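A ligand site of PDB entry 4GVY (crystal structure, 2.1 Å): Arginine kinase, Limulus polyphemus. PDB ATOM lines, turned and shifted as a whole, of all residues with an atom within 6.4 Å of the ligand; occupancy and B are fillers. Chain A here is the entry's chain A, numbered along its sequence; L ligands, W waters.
A nitrogen (N2) of the ligand lies within hydrogen-bond range of the side-chain carboxylate (OE1) of Glu 314, 2.5 Å away. OH of Tyr 68 lies within hydrogen-bond range of N1 of the ligand, 2.7 Å away. The backbone NH of Val 65 sits at hydrogen-bond distance from an oxygen (O2) of the ligand (2.7 Å). A ring nitrogen (NE2) of His 315 sits at hydrogen-bond distance from an oxygen (O1) of the ligand, at 2.9 Å. The backbone NH (N) of Gly 64 sits at hydrogen-bond distance from an oxygen (O1) of the ligand (2.9 Å). N of Gly 66 lies within hydrogen-bond range of O2 of the ligand (3.0 Å). O3 of the ligand sits at hydrogen-bond distance from NE2 of Gln 307 (3.1 Å).
The side-chain amide oxygen of Gln 307 sits at hydrogen-bond distance from the guanidinium group of Arg 309 (2.8 Å). The side-chain hydroxyl (OG1) of Thr 273 lies within hydrogen-bond range of the side-chain sulfur (SG) of Cys 271 (3.0 Å). The backbone carbonyl oxygen (O) of Thr 273 sits close to the guanidinium group (NE) of Arg 330 (3.2 Å).
The guanidinium group (NH2) of Arg 309 lies close to a nitrogen (N3) of the ligand (3.4 Å). Residues that only touch the ligand: Ser 63 and Thr 273. Hydrophobic or aromatic side chains within 4 Å of the ligand: Val 65, Tyr 68 and His 315. Ten residues have an atom within 4 Å of the ligand: Ser 63, Gly 64, Val 65, Gly 66, Tyr 68, Thr 273, Gln 307, Arg 309, Glu 314 and His 315.
Water W4 lies within hydrogen-bond range of the side-chain hydroxyl of Tyr 89 (2.6 Å), an oxygen (O3) of the ligand (2.6 Å), the guanidinium group of Arg 309 (3.0 Å), the side-chain amide oxygen of Gln 307 (3.3 Å) and the guanidinium group of Arg 330 (3.5 Å). Water W3 lies within hydrogen-bond range of N1 of the ligand, OG of Ser 63 and OG of Ser 56. Water W2 lies within hydrogen-bond range of the backbone carbonyl oxygen of Ile 67, a nitrogen (N1) of the ligand and the side-chain sulfur of Cys 271. Water W6 lies within hydrogen-bond range of the side-chain carboxylate of Glu 314 (2.6 Å) and a nitrogen (N2) of the ligand (3.0 Å). Water W1 bridges the backbone NH (N) of His 315 (3.2 Å) and a nitrogen (N3) of the ligand (3.5 Å).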
ATOM      1  N   SER A  25       0.501   6.476   0.999  1.00  0.00           N
ATOM      2  CA  SER A  25       0.019   7.798   0.596  1.00  0.00           C
ATOM      3  C   SER A  25       0.317   8.072  -0.872  1.00  0.00           C
ATOM      4  O   SER A  25       1.254   7.512  -1.443  1.00  0.00           O
ATOM      5  CB  SER A  25       0.661   8.891   1.461  1.00  0.00           C
ATOM      6  OG  SER A  25       2.067   8.957   1.262  1.00  0.00           O
ATOM      7  N   SER A  56       3.283  17.544   5.848  1.00  0.00           N
ATOM      8  CA  SER A  56       2.218  16.885   6.590  1.00  0.00           C
ATOM      9  C   SER A  56       2.260  15.389   6.288  1.00  0.00           C
ATOM     10  O   SER A  56       2.046  14.565   7.173  1.00  0.00           O
ATOM     11  CB  SER A  56       0.851  17.441   6.170  1.00  0.00           C
ATOM     12  OG  SER A  56      -0.194  16.752   6.843  1.00  0.00           O
ATOM     13  N   ASP A  62       0.672   7.861   7.612  1.00  0.00           N
ATOM     14  CA  ASP A  62      -0.635   7.249   7.387  1.00  0.00           C
ATOM     15  C   ASP A  62      -1.557   8.166   6.558  1.00  0.00           C
ATOM     16  O   ASP A  62      -2.729   7.835   6.352  1.00  0.00           O
ATOM     17  CB  ASP A  62      -1.271   6.849   8.720  1.00  0.00           C
ATOM     18  CG  ASP A  62      -1.464   8.026   9.656  1.00  0.00           C
ATOM     19  OD1 ASP A  62      -0.752   9.040   9.533  1.00  0.00           O
ATOM     20  OD2 ASP A  62      -2.340   7.909  10.540  1.00  0.00           O
ATOM     21  N   SER A  63      -1.045   9.310   6.129  1.00  0.00           N
ATOM     22  CA  SER A  63      -1.794  10.195   5.234  1.00  0.00           C
ATOM     23  C   SER A  63      -2.279   9.404   4.011  1.00  0.00           C
ATOM     24  O   SER A  63      -1.589   8.508   3.534  1.00  0.00           O
ATOM     25  CB  SER A  63      -0.949  11.388   4.772  1.00  0.00           C
ATOM     26  OG  SER A  63      -0.626  12.260   5.840  1.00  0.00           O
ATOM     27  N   GLY A  64      -3.463   9.742   3.502  1.00  0.00           N
ATOM     28  CA  GLY A  64      -3.904   9.210   2.236  1.00  0.00           C
ATOM     29  C   GLY A  64      -3.353   9.978   1.053  1.00  0.00           C
ATOM     30  O   GLY A  64      -3.097   9.405   0.002  1.00  0.00           O
ATOM     31  N   VAL A  65      -3.148  11.276   1.258  1.00  0.00           N
ATOM     32  CA  VAL A  65      -2.682  12.158   0.189  1.00  0.00           C
ATOM     33  C   VAL A  65      -1.328  12.747   0.555  1.00  0.00           C
ATOM     34  O   VAL A  65      -0.325  12.496  -0.114  1.00  0.00           O
ATOM     35  CB  VAL A  65      -3.685  13.278  -0.103  1.00  0.00           C
ATOM     36  CG1 VAL A  65      -3.149  14.212  -1.180  1.00  0.00           C
ATOM     37  CG2 VAL A  65      -5.040  12.698  -0.490  1.00  0.00           C
ATOM     38  N   GLY A  66      -1.300  13.561   1.613  1.00  0.00           N
ATOM     39  CA  GLY A  66      -0.050  13.990   2.202  1.00  0.00           C
ATOM     40  C   GLY A  66       0.477  15.355   1.807  1.00  0.00           C
ATOM     41  O   GLY A  66       1.527  15.767   2.282  1.00  0.00           O
ATOM     42  N   ILE A  67      -0.252  16.072   0.957  1.00  0.00           N
ATOM     43  CA  ILE A  67       0.199  17.399   0.538  1.00  0.00           C
ATOM     44  C   ILE A  67      -0.907  18.449   0.602  1.00  0.00           C
ATOM     45  O   ILE A  67      -2.099  18.132   0.564  1.00  0.00           O
ATOM     46  CB  ILE A  67       0.802  17.388  -0.891  1.00  0.00           C
ATOM     47  CG1 ILE A  67      -0.268  17.066  -1.924  1.00  0.00           C
ATOM     48  CG2 ILE A  67       1.983  16.427  -0.982  1.00  0.00           C
ATOM     49  CD1 ILE A  67       0.197  17.235  -3.346  1.00  0.00           C
ATOM     50  N   TYR A  68      -0.480  19.706   0.725  1.00  0.00           N
ATOM     51  CA  TYR A  68      -1.389  20.846   0.705  1.00  0.00           C
ATOM     52  C   TYR A  68      -0.719  21.977  -0.069  1.00  0.00           C
ATOM     53  O   TYR A  68       0.504  21.973  -0.239  1.00  0.00           O
ATOM     54  CB  TYR A  68      -1.631  21.330   2.138  1.00  0.00           C
ATOM     55  CG  TYR A  68      -2.403  20.378   3.026  1.00  0.00           C
ATOM     56  CD1 TYR A  68      -1.748  19.460   3.832  1.00  0.00           C
ATOM     57  CD2 TYR A  68      -3.789  20.420   3.074  1.00  0.00           C
ATOM     58  CE1 TYR A  68      -2.453  18.583   4.650  1.00  0.00           C
ATOM     59  CE2 TYR A  68      -4.503  19.555   3.892  1.00  0.00           C
ATOM     60  CZ  TYR A  68      -3.835  18.645   4.671  1.00  0.00           C
ATOM     61  OH  TYR A  68      -4.570  17.807   5.477  1.00  0.00           O
ATOM     62  N   TYR A  89      -6.119  11.012  -7.566  1.00  0.00           N
ATOM     63  CA  TYR A  89      -7.193  11.085  -6.574  1.00  0.00           C
ATOM     64  C   TYR A  89      -8.569  11.220  -7.242  1.00  0.00           C
ATOM     65  O   TYR A  89      -9.522  10.515  -6.890  1.00  0.00           O
ATOM     66  CB  TYR A  89      -6.979  12.253  -5.587  1.00  0.00           C
ATOM     67  CG  TYR A  89      -8.150  12.403  -4.638  1.00  0.00           C
ATOM     68  CD1 TYR A  89      -8.227  11.629  -3.486  1.00  0.00           C
ATOM     69  CD2 TYR A  89      -9.194  13.266  -4.919  1.00  0.00           C
ATOM     70  CE1 TYR A  89      -9.308  11.739  -2.623  1.00  0.00           C
ATOM     71  CE2 TYR A  89     -10.289  13.383  -4.071  1.00  0.00           C
ATOM     72  CZ  TYR A  89     -10.330  12.609  -2.926  1.00  0.00           C
ATOM     73  OH  TYR A  89     -11.413  12.708  -2.091  1.00  0.00           O
ATOM     74  N   PHE A 194      -2.926  16.188  10.811  1.00  0.00           N
ATOM     75  CA  PHE A 194      -2.574  16.388   9.415  1.00  0.00           C
ATOM     76  C   PHE A 194      -2.536  17.871   9.070  1.00  0.00           C
ATOM     77  O   PHE A 194      -1.617  18.337   8.390  1.00  0.00           O
ATOM     78  CB  PHE A 194      -3.566  15.644   8.522  1.00  0.00           C
ATOM     79  CG  PHE A 194      -3.617  14.168   8.794  1.00  0.00           C
ATOM     80  CD1 PHE A 194      -4.551  13.633   9.663  1.00  0.00           C
ATOM     81  CD2 PHE A 194      -2.695  13.309   8.197  1.00  0.00           C
ATOM     82  CE1 PHE A 194      -4.574  12.265   9.926  1.00  0.00           C
ATOM     83  CE2 PHE A 194      -2.714  11.943   8.452  1.00  0.00           C
ATOM     84  CZ  PHE A 194      -3.656  11.420   9.321  1.00  0.00           C
ATOM     85  N   LEU A 195      -3.506  18.616   9.583  1.00  0.00           N
ATOM     86  CA  LEU A 195      -3.561  20.059   9.365  1.00  0.00           C
ATOM     87  C   LEU A 195      -2.472  20.784  10.171  1.00  0.00           C
ATOM     88  O   LEU A 195      -1.854  21.734   9.694  1.00  0.00           O
ATOM     89  CB  LEU A 195      -4.947  20.596   9.750  1.00  0.00           C
ATOM     90  CG  LEU A 195      -6.068  20.256   8.779  1.00  0.00           C
ATOM     91  CD1 LEU A 195      -7.424  20.599   9.392  1.00  0.00           C
ATOM     92  CD2 LEU A 195      -5.863  20.962   7.434  1.00  0.00           C
ATOM     93  N   GLU A 225     -10.036  24.383   7.691  1.00  0.00           N
ATOM     94  CA  GLU A 225      -9.146  23.939   6.615  1.00  0.00           C
ATOM     95  C   GLU A 225      -9.201  24.923   5.446  1.00  0.00           C
ATOM     96  O   GLU A 225      -8.182  25.253   4.851  1.00  0.00           O
ATOM     97  CB  GLU A 225      -9.524  22.529   6.117  1.00  0.00           C
ATOM     98  CG  GLU A 225      -8.695  22.082   4.918  1.00  0.00           C
ATOM     99  CD  GLU A 225      -8.976  20.638   4.490  1.00  0.00           C
ATOM    100  OE1 GLU A 225      -8.775  20.347   3.298  1.00  0.00           O
ATOM    101  OE2 GLU A 225      -9.417  19.822   5.316  1.00  0.00           O
ATOM    102  N   CYS A 271      -6.526  21.946   0.194  1.00  0.00           N
ATOM    103  CA  CYS A 271      -6.153  20.576  -0.176  1.00  0.00           C
ATOM    104  C   CYS A 271      -6.533  20.314  -1.635  1.00  0.00           C
ATOM    105  O   CYS A 271      -7.585  20.748  -2.085  1.00  0.00           O
ATOM    106  CB  CYS A 271      -6.834  19.553   0.745  1.00  0.00           C
ATOM    107  SG  CYS A 271      -6.440  17.805   0.352  1.00  0.00           S
ATOM    108  N   THR A 273      -7.566  17.637  -2.900  1.00  0.00           N
ATOM    109  CA  THR A 273      -8.735  16.768  -2.983  1.00  0.00           C
ATOM    110  C   THR A 273     -10.023  17.570  -3.075  1.00  0.00           C
ATOM    111  O   THR A 273     -11.073  17.045  -3.449  1.00  0.00           O
ATOM    112  CB  THR A 273      -8.857  15.884  -1.727  1.00  0.00           C
ATOM    113  OG1 THR A 273      -9.080  16.710  -0.587  1.00  0.00           O
ATOM    114  CG2 THR A 273      -7.598  15.037  -1.535  1.00  0.00           C
ATOM    115  N   ASN A 274      -9.945  18.855  -2.751  1.00  0.00           N
ATOM    116  CA  ASN A 274     -11.142  19.692  -2.639  1.00  0.00           C
ATOM    117  C   ASN A 274     -11.335  20.680  -3.790  1.00  0.00           C
ATOM    118  O   ASN A 274     -12.201  21.545  -3.743  1.00  0.00           O
ATOM    119  CB  ASN A 274     -11.142  20.411  -1.290  1.00  0.00           C
ATOM    120  CG  ASN A 274     -11.499  19.486  -0.159  1.00  0.00           C
ATOM    121  OD1 ASN A 274     -12.418  18.676  -0.254  1.00  0.00           O
ATOM    122  ND2 ASN A 274     -10.724  19.550   0.913  1.00  0.00           N
ATOM    123  N   GLN A 307     -16.058   7.132  -1.090  1.00  0.00           N
ATOM    124  CA  GLN A 307     -15.074   7.006  -0.015  1.00  0.00           C
ATOM    125  C   GLN A 307     -15.783   6.694   1.301  1.00  0.00           C
ATOM    126  O   GLN A 307     -16.878   7.204   1.550  1.00  0.00           O
ATOM    127  CB  GLN A 307     -14.277   8.296   0.110  1.00  0.00           C
ATOM    128  CG  GLN A 307     -13.149   8.257   1.121  1.00  0.00           C
ATOM    129  CD  GLN A 307     -12.411   9.582   1.195  1.00  0.00           C
ATOM    130  OE1 GLN A 307     -12.994  10.598   1.555  1.00  0.00           O
ATOM    131  NE2 GLN A 307     -11.129   9.574   0.821  1.00  0.00           N
ATOM    132  N   ARG A 309     -15.531   6.904   5.469  1.00  0.00           N
ATOM    133  CA  ARG A 309     -14.871   7.523   6.625  1.00  0.00           C
ATOM    134  C   ARG A 309     -15.592   7.071   7.889  1.00  0.00           C
ATOM    135  O   ARG A 309     -16.731   6.608   7.829  1.00  0.00           O
ATOM    136  CB  ARG A 309     -14.960   9.049   6.511  1.00  0.00           C
ATOM    137  CG  ARG A 309     -14.201   9.618   5.327  1.00  0.00           C
ATOM    138  CD  ARG A 309     -14.445  11.109   5.197  1.00  0.00           C
ATOM    139  NE  ARG A 309     -13.764  11.639   4.020  1.00  0.00           N
ATOM    140  CZ  ARG A 309     -13.336  12.885   3.886  1.00  0.00           C
ATOM    141  NH1 ARG A 309     -13.566  13.781   4.837  1.00  0.00           N
ATOM    142  NH2 ARG A 309     -12.716  13.240   2.762  1.00  0.00           N
ATOM    143  N   GLU A 314     -13.095  11.933   8.681  1.00  0.00           N
ATOM    144  CA  GLU A 314     -11.920  11.223   8.173  1.00  0.00           C
ATOM    145  C   GLU A 314     -10.942  10.815   9.290  1.00  0.00           C
ATOM    146  O   GLU A 314     -10.889  11.463  10.328  1.00  0.00           O
ATOM    147  CB  GLU A 314     -11.189  12.081   7.141  1.00  0.00           C
ATOM    148  CG  GLU A 314     -10.793  13.444   7.677  1.00  0.00           C
ATOM    149  CD  GLU A 314      -9.848  14.170   6.750  1.00  0.00           C
ATOM    150  OE1 GLU A 314      -9.319  13.518   5.826  1.00  0.00           O
ATOM    151  OE2 GLU A 314      -9.625  15.384   6.947  1.00  0.00           O
ATOM    152  N   HIS A 315     -10.205   9.730   9.084  1.00  0.00           N
ATOM    153  CA  HIS A 315      -9.179   9.301  10.044  1.00  0.00           C
ATOM    154  C   HIS A 315      -9.769   8.866  11.376  1.00  0.00           C
ATOM    155  O   HIS A 315      -9.107   8.952  12.414  1.00  0.00           O
ATOM    156  CB  HIS A 315      -8.110  10.363  10.293  1.00  0.00           C
ATOM    157  CG  HIS A 315      -7.512  10.927   9.042  1.00  0.00           C
ATOM    158  ND1 HIS A 315      -7.509  12.281   8.765  1.00  0.00           N
ATOM    159  CD2 HIS A 315      -6.903  10.323   7.999  1.00  0.00           C
ATOM    160  CE1 HIS A 315      -6.918  12.484   7.598  1.00  0.00           C
ATOM    161  NE2 HIS A 315      -6.550  11.310   7.107  1.00  0.00           N
ATOM    162  N   ARG A 330     -14.103  15.386  -6.763  1.00  0.00           N
ATOM    163  CA  ARG A 330     -14.656  16.734  -6.672  1.00  0.00           C
ATOM    164  C   ARG A 330     -14.273  17.590  -7.882  1.00  0.00           C
ATOM    165  O   ARG A 330     -14.974  18.544  -8.223  1.00  0.00           O
ATOM    166  CB  ARG A 330     -14.156  17.405  -5.389  1.00  0.00           C
ATOM    167  CG  ARG A 330     -14.278  16.505  -4.173  1.00  0.00           C
ATOM    168  CD  ARG A 330     -14.240  17.286  -2.856  1.00  0.00           C
ATOM    169  NE  ARG A 330     -13.771  16.410  -1.778  1.00  0.00           N
ATOM    170  CZ  ARG A 330     -14.345  15.246  -1.455  1.00  0.00           C
ATOM    171  NH1 ARG A 330     -15.469  14.856  -2.062  1.00  0.00           N
ATOM    172  NH2 ARG A 330     -13.804  14.464  -0.531  1.00  0.00           N
HETATM  173  C1  LIG L   1      -4.514  12.898   4.279  1.00  0.00           C
HETATM  174  O1  LIG L   1      -4.983  11.864   4.776  1.00  0.00           O
HETATM  175  O2  LIG L   1      -3.669  12.966   3.363  1.00  0.00           O
HETATM  176  C2  LIG L   1      -5.024  14.310   4.852  1.00  0.00           C
HETATM  177  N1  LIG L   1      -4.108  15.354   4.374  1.00  0.00           N
HETATM  178  C3  LIG L   1      -6.468  14.537   4.297  1.00  0.00           C
HETATM  179  C4  LIG L   1      -6.630  14.379   2.768  1.00  0.00           C
HETATM  180  C5  LIG L   1      -8.152  14.316   2.379  1.00  0.00           C
HETATM  181  N2  LIG L   1      -8.920  13.474   3.318  1.00  0.00           N
HETATM  182  C6  LIG L   1      -9.330  12.200   2.978  1.00  0.00           C
HETATM  183  O3  LIG L   1      -9.107  11.681   1.848  1.00  0.00           O
HETATM  184  N3  LIG L   1     -10.030  11.442   3.907  1.00  0.00           N
HETATM  185  O   HOH W   1     -10.284   8.744   6.048  1.00  0.00           O
HETATM  186  O   HOH W   2      -3.885  16.376   1.570  1.00  0.00           O
HETATM  187  O   HOH W   3      -1.515  14.804   5.173  1.00  0.00           O
HETATM  188  O   HOH W   4     -10.878  12.854   0.399  1.00  0.00           O
HETATM  189  O   HOH W   5      -7.308   9.849   1.750  1.00  0.00           O
HETATM  190  O   HOH W   6      -9.559  16.218   4.480  1.00  0.00           O
